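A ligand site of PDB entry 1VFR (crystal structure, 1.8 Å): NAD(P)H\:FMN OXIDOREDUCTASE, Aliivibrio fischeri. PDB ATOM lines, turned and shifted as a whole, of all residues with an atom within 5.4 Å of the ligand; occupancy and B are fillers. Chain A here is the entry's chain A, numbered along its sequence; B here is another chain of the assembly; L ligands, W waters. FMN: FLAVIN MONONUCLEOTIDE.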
ATOM      1  N   ARG A  12      -9.225  16.897 -20.283  1.00  0.00           N
ATOM      2  CA  ARG A  12      -9.916  17.182 -19.033  1.00  0.00           C
ATOM      3  C   ARG A  12     -10.391  15.824 -18.530  1.00  0.00           C
ATOM      4  O   ARG A  12     -10.552  14.886 -19.311  1.00  0.00           O
ATOM      5  CB  ARG A  12     -11.096  18.135 -19.231  1.00  0.00           C
ATOM      6  CG  ARG A  12     -12.224  17.582 -20.113  1.00  0.00           C
ATOM      7  CD  ARG A  12     -13.603  18.070 -19.649  1.00  0.00           C
ATOM      8  NE  ARG A  12     -13.950  17.539 -18.320  1.00  0.00           N
ATOM      9  CZ  ARG A  12     -14.283  16.273 -18.043  1.00  0.00           C
ATOM     10  NH1 ARG A  12     -14.324  15.340 -18.986  1.00  0.00           N
ATOM     11  NH2 ARG A  12     -14.502  15.921 -16.786  1.00  0.00           N
ATOM     12  N   TYR A  13     -10.565  15.703 -17.208  1.00  0.00           N
ATOM     13  CA  TYR A  13     -10.998  14.449 -16.608  1.00  0.00           C
ATOM     14  C   TYR A  13     -11.450  14.745 -15.181  1.00  0.00           C
ATOM     15  O   TYR A  13     -11.287  15.871 -14.685  1.00  0.00           O
ATOM     16  CB  TYR A  13      -9.830  13.437 -16.576  1.00  0.00           C
ATOM     17  CG  TYR A  13      -8.774  13.765 -15.544  1.00  0.00           C
ATOM     18  CD1 TYR A  13      -7.928  14.867 -15.715  1.00  0.00           C
ATOM     19  CD2 TYR A  13      -8.665  13.026 -14.366  1.00  0.00           C
ATOM     20  CE1 TYR A  13      -7.019  15.215 -14.718  1.00  0.00           C
ATOM     21  CE2 TYR A  13      -7.760  13.359 -13.385  1.00  0.00           C
ATOM     22  CZ  TYR A  13      -6.955  14.453 -13.563  1.00  0.00           C
ATOM     23  OH  TYR A  13      -6.091  14.814 -12.580  1.00  0.00           O
ATOM     24  N   THR A  14     -12.021  13.734 -14.543  1.00  0.00           N
ATOM     25  CA  THR A  14     -12.486  13.872 -13.157  1.00  0.00           C
ATOM     26  C   THR A  14     -11.358  13.552 -12.183  1.00  0.00           C
ATOM     27  O   THR A  14     -10.906  12.412 -12.058  1.00  0.00           O
ATOM     28  CB  THR A  14     -13.731  12.975 -12.879  1.00  0.00           C
ATOM     29  OG1 THR A  14     -14.821  13.408 -13.721  1.00  0.00           O
ATOM     30  CG2 THR A  14     -14.170  13.068 -11.402  1.00  0.00           C
ATOM     31  N   SER A  15     -10.867  14.575 -11.519  1.00  0.00           N
ATOM     32  CA  SER A  15      -9.796  14.403 -10.563  1.00  0.00           C
ATOM     33  C   SER A  15     -10.301  13.647  -9.330  1.00  0.00           C
ATOM     34  O   SER A  15     -11.411  13.858  -8.871  1.00  0.00           O
ATOM     35  CB  SER A  15      -9.234  15.784 -10.189  1.00  0.00           C
ATOM     36  OG  SER A  15      -8.216  15.656  -9.216  1.00  0.00           O
ATOM     37  N   LYS A  16      -9.474  12.734  -8.818  1.00  0.00           N
ATOM     38  CA  LYS A  16      -9.841  11.932  -7.635  1.00  0.00           C
ATOM     39  C   LYS A  16      -9.008  12.273  -6.386  1.00  0.00           C
ATOM     40  O   LYS A  16      -9.092  11.581  -5.376  1.00  0.00           O
ATOM     41  CB  LYS A  16      -9.676  10.439  -7.960  1.00  0.00           C
ATOM     42  CG  LYS A  16     -10.542   9.955  -9.109  1.00  0.00           C
ATOM     43  CD  LYS A  16     -12.044  10.003  -8.791  1.00  0.00           C
ATOM     44  CE  LYS A  16     -12.863   9.593 -10.010  1.00  0.00           C
ATOM     45  NZ  LYS A  16     -14.322   9.512  -9.714  1.00  0.00           N
ATOM     46  N   PHE A  72     -17.295   9.338   0.156  1.00  0.00           N
ATOM     47  CA  PHE A  72     -16.171   9.191  -0.770  1.00  0.00           C
ATOM     48  C   PHE A  72     -15.804  10.534  -1.418  1.00  0.00           C
ATOM     49  O   PHE A  72     -14.674  10.735  -1.858  1.00  0.00           O
ATOM     50  CB  PHE A  72     -16.438   8.124  -1.833  1.00  0.00           C
ATOM     51  CG  PHE A  72     -17.462   8.517  -2.880  1.00  0.00           C
ATOM     52  CD1 PHE A  72     -18.815   8.657  -2.558  1.00  0.00           C
ATOM     53  CD2 PHE A  72     -17.073   8.716  -4.206  1.00  0.00           C
ATOM     54  CE1 PHE A  72     -19.751   8.976  -3.538  1.00  0.00           C
ATOM     55  CE2 PHE A  72     -18.003   9.034  -5.194  1.00  0.00           C
ATOM     56  CZ  PHE A  72     -19.357   9.168  -4.860  1.00  0.00           C
ATOM     57  N   ASN A  73     -16.756  11.454  -1.445  1.00  0.00           N
ATOM     58  CA  ASN A  73     -16.519  12.774  -2.005  1.00  0.00           C
ATOM     59  C   ASN A  73     -16.035  13.777  -0.963  1.00  0.00           C
ATOM     60  O   ASN A  73     -15.533  14.861  -1.308  1.00  0.00           O
ATOM     61  CB  ASN A  73     -17.798  13.327  -2.621  1.00  0.00           C
ATOM     62  CG  ASN A  73     -18.098  12.759  -3.991  1.00  0.00           C
ATOM     63  OD1 ASN A  73     -17.192  12.368  -4.734  1.00  0.00           O
ATOM     64  ND2 ASN A  73     -19.369  12.767  -4.356  1.00  0.00           N
ATOM     65  N   HIS A  76     -12.278  15.784  -0.747  1.00  0.00           N
ATOM     66  CA  HIS A  76     -11.968  16.840  -1.704  1.00  0.00           C
ATOM     67  C   HIS A  76     -12.312  18.237  -1.197  1.00  0.00           C
ATOM     68  O   HIS A  76     -11.696  19.210  -1.636  1.00  0.00           O
ATOM     69  CB  HIS A  76     -12.757  16.659  -3.003  1.00  0.00           C
ATOM     70  CG  HIS A  76     -12.618  15.298  -3.621  1.00  0.00           C
ATOM     71  ND1 HIS A  76     -11.429  14.622  -3.656  1.00  0.00           N
ATOM     72  CD2 HIS A  76     -13.539  14.499  -4.219  1.00  0.00           C
ATOM     73  CE1 HIS A  76     -11.607  13.448  -4.241  1.00  0.00           C
ATOM     74  NE2 HIS A  76     -12.879  13.351  -4.587  1.00  0.00           N
ATOM     75  N   TYR A 144     -27.761  22.137 -15.310  1.00  0.00           N
ATOM     76  CA  TYR A 144     -26.839  21.160 -15.886  1.00  0.00           C
ATOM     77  C   TYR A 144     -26.216  21.693 -17.190  1.00  0.00           C
ATOM     78  O   TYR A 144     -25.092  21.325 -17.536  1.00  0.00           O
ATOM     79  CB  TYR A 144     -27.524  19.802 -16.117  1.00  0.00           C
ATOM     80  CG  TYR A 144     -27.447  18.916 -14.904  1.00  0.00           C
ATOM     81  CD1 TYR A 144     -28.127  19.255 -13.714  1.00  0.00           C
ATOM     82  CD2 TYR A 144     -26.703  17.739 -14.922  1.00  0.00           C
ATOM     83  CE1 TYR A 144     -28.042  18.442 -12.591  1.00  0.00           C
ATOM     84  CE2 TYR A 144     -26.617  16.918 -13.811  1.00  0.00           C
ATOM     85  CZ  TYR A 144     -27.295  17.284 -12.647  1.00  0.00           C
ATOM     86  OH  TYR A 144     -27.212  16.454 -11.564  1.00  0.00           O
ATOM     87  N   LEU A 147     -23.516  23.746 -16.077  1.00  0.00           N
ATOM     88  CA  LEU A 147     -22.423  22.879 -15.629  1.00  0.00           C
ATOM     89  C   LEU A 147     -21.602  22.390 -16.834  1.00  0.00           C
ATOM     90  O   LEU A 147     -20.367  22.330 -16.761  1.00  0.00           O
ATOM     91  CB  LEU A 147     -22.956  21.694 -14.829  1.00  0.00           C
ATOM     92  CG  LEU A 147     -22.009  20.570 -14.413  1.00  0.00           C
ATOM     93  CD1 LEU A 147     -20.872  21.075 -13.507  1.00  0.00           C
ATOM     94  CD2 LEU A 147     -22.809  19.494 -13.677  1.00  0.00           C
ATOM     95  N   LEU A 151     -17.572  22.962 -17.302  1.00  0.00           N
ATOM     96  CA  LEU A 151     -16.562  21.944 -17.510  1.00  0.00           C
ATOM     97  C   LEU A 151     -15.713  22.254 -18.738  1.00  0.00           C
ATOM     98  O   LEU A 151     -14.506  22.034 -18.732  1.00  0.00           O
ATOM     99  CB  LEU A 151     -17.224  20.578 -17.615  1.00  0.00           C
ATOM    100  CG  LEU A 151     -17.802  20.032 -16.298  1.00  0.00           C
ATOM    101  CD1 LEU A 151     -18.539  18.740 -16.603  1.00  0.00           C
ATOM    102  CD2 LEU A 151     -16.680  19.787 -15.255  1.00  0.00           C
ATOM    103  N   THR A 162     -13.831  18.157 -10.131  1.00  0.00           N
ATOM    104  CA  THR A 162     -14.559  16.938  -9.787  1.00  0.00           C
ATOM    105  C   THR A 162     -16.028  17.301  -9.657  1.00  0.00           C
ATOM    106  O   THR A 162     -16.411  18.034  -8.750  1.00  0.00           O
ATOM    107  CB  THR A 162     -14.097  16.351  -8.420  1.00  0.00           C
ATOM    108  OG1 THR A 162     -12.677  16.217  -8.407  1.00  0.00           O
ATOM    109  CG2 THR A 162     -14.739  14.949  -8.176  1.00  0.00           C
ATOM    110  N   THR A 163     -16.849  16.857 -10.599  1.00  0.00           N
ATOM    111  CA  THR A 163     -18.281  17.102 -10.549  1.00  0.00           C
ATOM    112  C   THR A 163     -18.791  16.115  -9.504  1.00  0.00           C
ATOM    113  O   THR A 163     -18.290  14.994  -9.404  1.00  0.00           O
ATOM    114  CB  THR A 163     -18.954  16.797 -11.900  1.00  0.00           C
ATOM    115  OG1 THR A 163     -18.275  17.508 -12.942  1.00  0.00           O
ATOM    116  CG2 THR A 163     -20.401  17.238 -11.888  1.00  0.00           C
ATOM    117  N   MET A 164     -19.799  16.529  -8.718  1.00  0.00           N
ATOM    118  CA  MET A 164     -20.297  15.648  -7.683  1.00  0.00           C
ATOM    119  C   MET A 164     -21.807  15.602  -7.525  1.00  0.00           C
ATOM    120  O   MET A 164     -22.431  16.607  -7.169  1.00  0.00           O
ATOM    121  CB  MET A 164     -19.683  16.031  -6.321  1.00  0.00           C
ATOM    122  CG  MET A 164     -18.179  15.916  -6.212  1.00  0.00           C
ATOM    123  SD  MET A 164     -17.507  16.519  -4.615  1.00  0.00           S
ATOM    124  CE  MET A 164     -18.037  18.152  -4.665  1.00  0.00           C
ATOM    125  N   GLU A 165     -22.401  14.445  -7.820  1.00  0.00           N
ATOM    126  CA  GLU A 165     -23.834  14.245  -7.614  1.00  0.00           C
ATOM    127  C   GLU A 165     -23.953  13.494  -6.287  1.00  0.00           C
ATOM    128  O   GLU A 165     -25.041  13.314  -5.745  1.00  0.00           O
ATOM    129  CB  GLU A 165     -24.467  13.401  -8.740  1.00  0.00           C
ATOM    130  CG  GLU A 165     -25.210  14.240  -9.782  1.00  0.00           C
ATOM    131  CD  GLU A 165     -25.851  13.376 -10.888  1.00  0.00           C
ATOM    132  OE1 GLU A 165     -25.837  12.135 -10.790  1.00  0.00           O
ATOM    133  OE2 GLU A 165     -26.391  13.979 -11.849  1.00  0.00           O
ATOM    134  N   GLY A 166     -22.819  12.997  -5.800  1.00  0.00           N
ATOM    135  CA  GLY A 166     -22.764  12.270  -4.549  1.00  0.00           C
ATOM    136  C   GLY A 166     -22.706  13.271  -3.411  1.00  0.00           C
ATOM    137  O   GLY A 166     -21.678  13.422  -2.749  1.00  0.00           O
ATOM    138  N   VAL A 187     -26.140  19.031  -7.553  1.00  0.00           N
ATOM    139  CA  VAL A 187     -24.803  18.816  -8.081  1.00  0.00           C
ATOM    140  C   VAL A 187     -23.869  19.945  -7.649  1.00  0.00           C
ATOM    141  O   VAL A 187     -24.277  21.105  -7.554  1.00  0.00           O
ATOM    142  CB  VAL A 187     -24.832  18.661  -9.640  1.00  0.00           C
ATOM    143  CG1 VAL A 187     -25.310  19.948 -10.297  1.00  0.00           C
ATOM    144  CG2 VAL A 187     -23.476  18.212 -10.165  1.00  0.00           C
ATOM    145  N   ASN A 201      -6.628   8.798 -11.301  1.00  0.00           N
ATOM    146  CA  ASN A 201      -7.391   8.989 -12.521  1.00  0.00           C
ATOM    147  C   ASN A 201      -6.660   9.827 -13.566  1.00  0.00           C
ATOM    148  O   ASN A 201      -7.045   9.831 -14.727  1.00  0.00           O
ATOM    149  CB  ASN A 201      -8.746   9.597 -12.202  1.00  0.00           C
ATOM    150  CG  ASN A 201      -9.788   9.179 -13.191  1.00  0.00           C
ATOM    151  OD1 ASN A 201      -9.705   8.103 -13.781  1.00  0.00           O
ATOM    152  ND2 ASN A 201     -10.789  10.025 -13.386  1.00  0.00           N
ATOM    153  N   LYS A 206      -9.229   7.752 -21.027  1.00  0.00           N
ATOM    154  CA  LYS A 206     -10.629   8.171 -21.013  1.00  0.00           C
ATOM    155  C   LYS A 206     -11.395   7.125 -21.833  1.00  0.00           C
ATOM    156  O   LYS A 206     -10.878   6.586 -22.821  1.00  0.00           O
ATOM    157  CB  LYS A 206     -10.804   9.573 -21.641  1.00  0.00           C
ATOM    158  CG  LYS A 206     -12.225  10.132 -21.535  1.00  0.00           C
ATOM    159  CD  LYS A 206     -12.347  11.572 -21.988  1.00  0.00           C
ATOM    160  CE  LYS A 206     -11.398  12.475 -21.200  1.00  0.00           C
ATOM    161  NZ  LYS A 206     -11.621  12.412 -19.727  1.00  0.00           N
ATOM    162  N   ARG A 208     -15.251   6.268 -23.599  1.00  0.00           N
ATOM    163  CA  ARG A 208     -16.575   6.682 -24.034  1.00  0.00           C
ATOM    164  C   ARG A 208     -17.100   5.634 -25.016  1.00  0.00           C
ATOM    165  O   ARG A 208     -16.326   4.864 -25.573  1.00  0.00           O
ATOM    166  CB  ARG A 208     -16.497   8.035 -24.759  1.00  0.00           C
ATOM    167  CG  ARG A 208     -16.181   9.222 -23.846  1.00  0.00           C
ATOM    168  CD  ARG A 208     -17.261   9.433 -22.780  1.00  0.00           C
ATOM    169  NE  ARG A 208     -17.042  10.692 -22.085  1.00  0.00           N
ATOM    170  CZ  ARG A 208     -16.233  10.836 -21.058  1.00  0.00           C
ATOM    171  NH1 ARG A 208     -15.578   9.802 -20.567  1.00  0.00           N
ATOM    172  NH2 ARG A 208     -16.013  12.055 -20.558  1.00  0.00           N
ATOM    173  N   LEU B  38     -17.465  13.123 -26.205  1.00  0.00           N
ATOM    174  CA  LEU B  38     -16.552  13.259 -25.060  1.00  0.00           C
ATOM    175  C   LEU B  38     -17.162  13.919 -23.829  1.00  0.00           C
ATOM    176  O   LEU B  38     -16.491  14.035 -22.812  1.00  0.00           O
ATOM    177  CB  LEU B  38     -15.304  14.020 -25.486  1.00  0.00           C
ATOM    178  CG  LEU B  38     -14.439  13.293 -26.521  1.00  0.00           C
ATOM    179  CD1 LEU B  38     -13.344  14.221 -26.995  1.00  0.00           C
ATOM    180  CD2 LEU B  38     -13.845  12.038 -25.924  1.00  0.00           C
ATOM    181  N   ALA B  40     -18.984  14.648 -20.345  1.00  0.00           N
ATOM    182  CA  ALA B  40     -18.987  13.920 -19.091  1.00  0.00           C
ATOM    183  C   ALA B  40     -20.428  13.648 -18.675  1.00  0.00           C
ATOM    184  O   ALA B  40     -21.339  14.355 -19.076  1.00  0.00           O
ATOM    185  CB  ALA B  40     -18.263  14.734 -18.003  1.00  0.00           C
ATOM    186  N   SER B  41     -20.621  12.634 -17.846  1.00  0.00           N
ATOM    187  CA  SER B  41     -21.953  12.317 -17.347  1.00  0.00           C
ATOM    188  C   SER B  41     -21.785  11.542 -16.063  1.00  0.00           C
ATOM    189  O   SER B  41     -20.725  10.959 -15.831  1.00  0.00           O
ATOM    190  CB  SER B  41     -22.747  11.493 -18.375  1.00  0.00           C
ATOM    191  OG  SER B  41     -22.099  10.271 -18.671  1.00  0.00           O
ATOM    192  N   SER B  42     -22.809  11.578 -15.215  1.00  0.00           N
ATOM    193  CA  SER B  42     -22.773  10.866 -13.942  1.00  0.00           C
ATOM    194  C   SER B  42     -22.484   9.397 -14.228  1.00  0.00           C
ATOM    195  O   SER B  42     -23.103   8.801 -15.093  1.00  0.00           O
ATOM    196  CB  SER B  42     -24.110  11.029 -13.226  1.00  0.00           C
ATOM    197  OG  SER B  42     -24.035  10.445 -11.941  1.00  0.00           O
ATOM    198  N   ILE B  43     -21.517   8.844 -13.498  1.00  0.00           N
ATOM    199  CA  ILE B  43     -21.019   7.463 -13.610  1.00  0.00           C
ATOM    200  C   ILE B  43     -20.635   7.003 -15.046  1.00  0.00           C
ATOM    201  O   ILE B  43     -20.471   5.805 -15.310  1.00  0.00           O
ATOM    202  CB  ILE B  43     -21.930   6.395 -12.864  1.00  0.00           C
ATOM    203  CG1 ILE B  43     -23.251   6.125 -13.612  1.00  0.00           C
ATOM    204  CG2 ILE B  43     -22.220   6.895 -11.454  1.00  0.00           C
ATOM    205  CD1 ILE B  43     -23.963   4.833 -13.184  1.00  0.00           C
ATOM    206  N   ASN B  44     -20.350   7.972 -15.914  1.00  0.00           N
ATOM    207  CA  ASN B  44     -20.009   7.706 -17.321  1.00  0.00           C
ATOM    208  C   ASN B  44     -21.150   6.931 -17.989  1.00  0.00           C
ATOM    209  O   ASN B  44     -20.953   6.202 -18.951  1.00  0.00           O
ATOM    210  CB  ASN B  44     -18.689   6.933 -17.449  1.00  0.00           C
ATOM    211  CG  ASN B  44     -18.030   7.136 -18.820  1.00  0.00           C
ATOM    212  OD1 ASN B  44     -18.289   8.116 -19.509  1.00  0.00           O
ATOM    213  ND2 ASN B  44     -17.182   6.198 -19.224  1.00  0.00           N
ATOM    214  N   PHE B 124     -26.272   4.921  -7.929  1.00  0.00           N
ATOM    215  CA  PHE B 124     -26.743   6.211  -8.410  1.00  0.00           C
ATOM    216  C   PHE B 124     -27.938   6.102  -9.336  1.00  0.00           C
ATOM    217  O   PHE B 124     -28.801   6.980  -9.336  1.00  0.00           O
ATOM    218  CB  PHE B 124     -25.632   6.984  -9.111  1.00  0.00           C
ATOM    219  CG  PHE B 124     -24.610   7.535  -8.161  1.00  0.00           C
ATOM    220  CD1 PHE B 124     -23.498   6.783  -7.796  1.00  0.00           C
ATOM    221  CD2 PHE B 124     -24.757   8.819  -7.638  1.00  0.00           C
ATOM    222  CE1 PHE B 124     -22.545   7.295  -6.904  1.00  0.00           C
ATOM    223  CE2 PHE B 124     -23.804   9.345  -6.746  1.00  0.00           C
ATOM    224  CZ  PHE B 124     -22.698   8.586  -6.385  1.00  0.00           C
ATOM    225  N   GLN B 142     -28.360  14.973 -17.802  1.00  0.00           N
ATOM    226  CA  GLN B 142     -27.074  14.583 -18.391  1.00  0.00           C
ATOM    227  C   GLN B 142     -26.976  15.044 -19.850  1.00  0.00           C
ATOM    228  O   GLN B 142     -25.909  15.463 -20.305  1.00  0.00           O
ATOM    229  CB  GLN B 142     -26.835  13.064 -18.334  1.00  0.00           C
ATOM    230  CG  GLN B 142     -27.146  12.383 -17.005  1.00  0.00           C
ATOM    231  CD  GLN B 142     -26.340  12.904 -15.843  1.00  0.00           C
ATOM    232  OE1 GLN B 142     -25.127  13.089 -15.934  1.00  0.00           O
ATOM    233  NE2 GLN B 142     -27.007  13.125 -14.727  1.00  0.00           N
ATOM    234  N   LEU B 145     -26.229  18.688 -20.018  1.00  0.00           N
ATOM    235  CA  LEU B 145     -24.817  18.936 -19.757  1.00  0.00           C
ATOM    236  C   LEU B 145     -24.115  18.863 -21.129  1.00  0.00           C
ATOM    237  O   LEU B 145     -23.333  19.742 -21.473  1.00  0.00           O
ATOM    238  CB  LEU B 145     -24.238  17.892 -18.817  1.00  0.00           C
ATOM    239  CG  LEU B 145     -22.830  18.137 -18.257  1.00  0.00           C
ATOM    240  CD1 LEU B 145     -22.645  17.267 -17.018  1.00  0.00           C
ATOM    241  CD2 LEU B 145     -21.730  17.835 -19.287  1.00  0.00           C
HETATM  242  N1  FMN L   1     -17.198  11.675  -9.828  1.00  0.00           N
HETATM  243  C2  FMN L   1     -16.876  11.597  -8.479  1.00  0.00           C
HETATM  244  O2  FMN L   1     -15.807  11.172  -8.105  1.00  0.00           O
HETATM  245  N3  FMN L   1     -17.982  11.775  -7.632  1.00  0.00           N
HETATM  246  C4  FMN L   1     -19.270  12.144  -8.007  1.00  0.00           C
HETATM  247  O4  FMN L   1     -20.129  12.301  -7.131  1.00  0.00           O
HETATM  248  C4A FMN L   1     -19.439  12.244  -9.450  1.00  0.00           C
HETATM  249  N5  FMN L   1     -20.659  12.716  -9.878  1.00  0.00           N
HETATM  250  C5A FMN L   1     -20.838  13.130 -11.163  1.00  0.00           C
HETATM  251  C6  FMN L   1     -22.004  13.741 -11.500  1.00  0.00           C
HETATM  252  C7  FMN L   1     -22.126  14.255 -12.770  1.00  0.00           C
HETATM  253  C7M FMN L   1     -23.398  14.963 -13.163  1.00  0.00           C
HETATM  254  C8  FMN L   1     -21.053  14.165 -13.704  1.00  0.00           C
HETATM  255  C8M FMN L   1     -21.060  14.880 -15.044  1.00  0.00           C
HETATM  256  C9  FMN L   1     -19.933  13.482 -13.375  1.00  0.00           C
HETATM  257  C9A FMN L   1     -19.788  12.961 -12.099  1.00  0.00           C
HETATM  258  N10 FMN L   1     -18.615  12.381 -11.706  1.00  0.00           N
HETATM  259  C10 FMN L   1     -18.387  12.068 -10.397  1.00  0.00           C
HETATM  260  C1' FMN L   1     -17.587  12.088 -12.587  1.00  0.00           C
HETATM  261  C2' FMN L   1     -17.927  11.096 -13.690  1.00  0.00           C
HETATM  262  O2' FMN L   1     -17.766   9.809 -13.173  1.00  0.00           O
HETATM  263  C3' FMN L   1     -17.057  11.355 -14.951  1.00  0.00           C
HETATM  264  O3' FMN L   1     -17.415  12.650 -15.466  1.00  0.00           O
HETATM  265  C4' FMN L   1     -17.327  10.285 -16.055  1.00  0.00           C
HETATM  266  O4' FMN L   1     -16.811   9.018 -15.551  1.00  0.00           O
HETATM  267  C5' FMN L   1     -16.495  10.638 -17.288  1.00  0.00           C
HETATM  268  O5' FMN L   1     -15.060  10.812 -16.951  1.00  0.00           O
HETATM  269  P   FMN L   1     -14.163  12.130 -17.063  1.00  0.00           P
HETATM  270  O1P FMN L   1     -12.981  11.565 -16.399  1.00  0.00           O
HETATM  271  O2P FMN L   1     -15.027  13.099 -16.358  1.00  0.00           O
HETATM  272  O3P FMN L   1     -14.165  12.316 -18.487  1.00  0.00           O
HETATM  273  O   HOH W   1     -13.308   9.486 -14.895  1.00  0.00           O
HETATM  274  O   HOH W   2     -19.803   9.328 -11.001  1.00  0.00           O
HETATM  275  O   HOH W   3     -14.659  11.370  -5.549  1.00  0.00           O
HETATM  276  O   HOH W   4     -11.333  10.184 -17.964  1.00  0.00           O
HETATM  277  O   HOH W   5     -15.060   9.248 -12.560  1.00  0.00           O
HETATM  278  O   HOH W   6     -14.853   7.261 -16.499  1.00  0.00           O
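The guanidinium group (NH2) of Arg 12 lies within salt-bridge range of an oxygen (O2P) of the ligand (2.9 Å).
The backbone NH of Gly 166 lies within hydrogen-bond range of an oxygen (O4) of the ligand (3.1 Å).
OG1 of Thr 14 is in hydrogen-bond range of O2P of the ligand, 2.7 Å away.
The guanidinium group of Arg 208 is in salt-bridge range of an oxygen (O3P) of the ligand (2.8 Å).
An oxygen (O4) of the ligand lies within hydrogen-bond range of the side-chain amide nitrogen of Asn 73.
The backbone NH (N) of Thr 14 sits at hydrogen-bond distance from an oxygen (O1P) of the ligand, 3.0 Å away.
The side-chain amino group (NZ) of Lys 206 is in salt-bridge range of an oxygen (O3P) of the ligand, at 2.8 Å.
The backbone NH of Glu 165 sits at hydrogen-bond distance from an oxygen (O4) of the ligand (3.2 Å).
The side-chain amino group (NZ) of Lys 16 is in hydrogen-bond range of an oxygen (O2) of the ligand (2.7 Å).
N of Ser 42 of chain B sits at hydrogen-bond distance from OE1 of Gln 142 of chain B (2.9 Å).
OH of Tyr 144 lies within hydrogen-bond range of OE2 of Glu 165.
O of Arg 12 is in hydrogen-bond range of NZ of Lys 206 (2.7 Å).
The guanidinium group (NH1) of Arg 208 is in hydrogen-bond range of the side-chain amide oxygen (OD1) of Asn 44 of chain B (3.4 Å).
The backbone carbonyl oxygen of Ser 15 is in hydrogen-bond range of the side-chain hydroxyl of Thr 162 (2.7 Å).
ND2 of Asn 73 is in hydrogen-bond range of O of Gly 166 (2.9 Å).
The side-chain carboxylate (OE2) of Glu 165 sits at hydrogen-bond distance from the side-chain amide nitrogen (NE2) of Gln 142 of chain B (3.1 Å).
The guanidinium group of Arg 208 is in hydrogen-bond range of the backbone carbonyl oxygen of Leu 38 of chain B, 3.0 Å away.
The backbone carbonyl oxygen (O) of Thr 163 sits close to a nitrogen (N5) of the ligand.
Residues that only touch the ligand: Asn 44 of chain B (3.4 Å), Ala 40 of chain B (3.4 Å), Met 164 (3.4 Å), Ser 41 of chain B (3.5 Å), Ser 42 of chain B (3.5 Å), Leu 145 of chain B (3.5 Å), Tyr 13 (3.5 Å), Phe 72 (3.7 Å), Gln 142 of chain B (3.8 Å), Tyr 144 (3.8 Å), Ile 43 of chain B (3.9 Å) and Thr 162 (3.9 Å).
Hydrophobic or aromatic side chains within 4 Å of the ligand: Tyr 13, Phe 72, Tyr 144, Met 164, Ala 40 of chain B and Leu 145 of chain B.
Of the 29 residues printed, 21 come within 4 Å of the ligand.
The nearest printed residue that does not touch the ligand is Asn 201 (4.03 Å).
Water W1 bridges O1P of the ligand and ND2 of Asn 201.
Water W4 lies within hydrogen-bond range of O1P of the ligand (2.7 Å) and NZ of Lys 206 (2.9 Å).
Water W3 lies within hydrogen-bond range of an oxygen (O2) of the ligand (2.8 Å), a ring nitrogen (NE2) of His 76 (2.8 Å) and the side-chain amide oxygen (OD1) of Asn 73 (2.8 Å).
Water W5 lies within hydrogen-bond range of O2' of the ligand (2.8 Å) and NZ of Lys 16 (3.0 Å).
Water W2 bridges O2' of the ligand (3.0 Å) and N of Ile 43 of chain B (3.1 Å).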
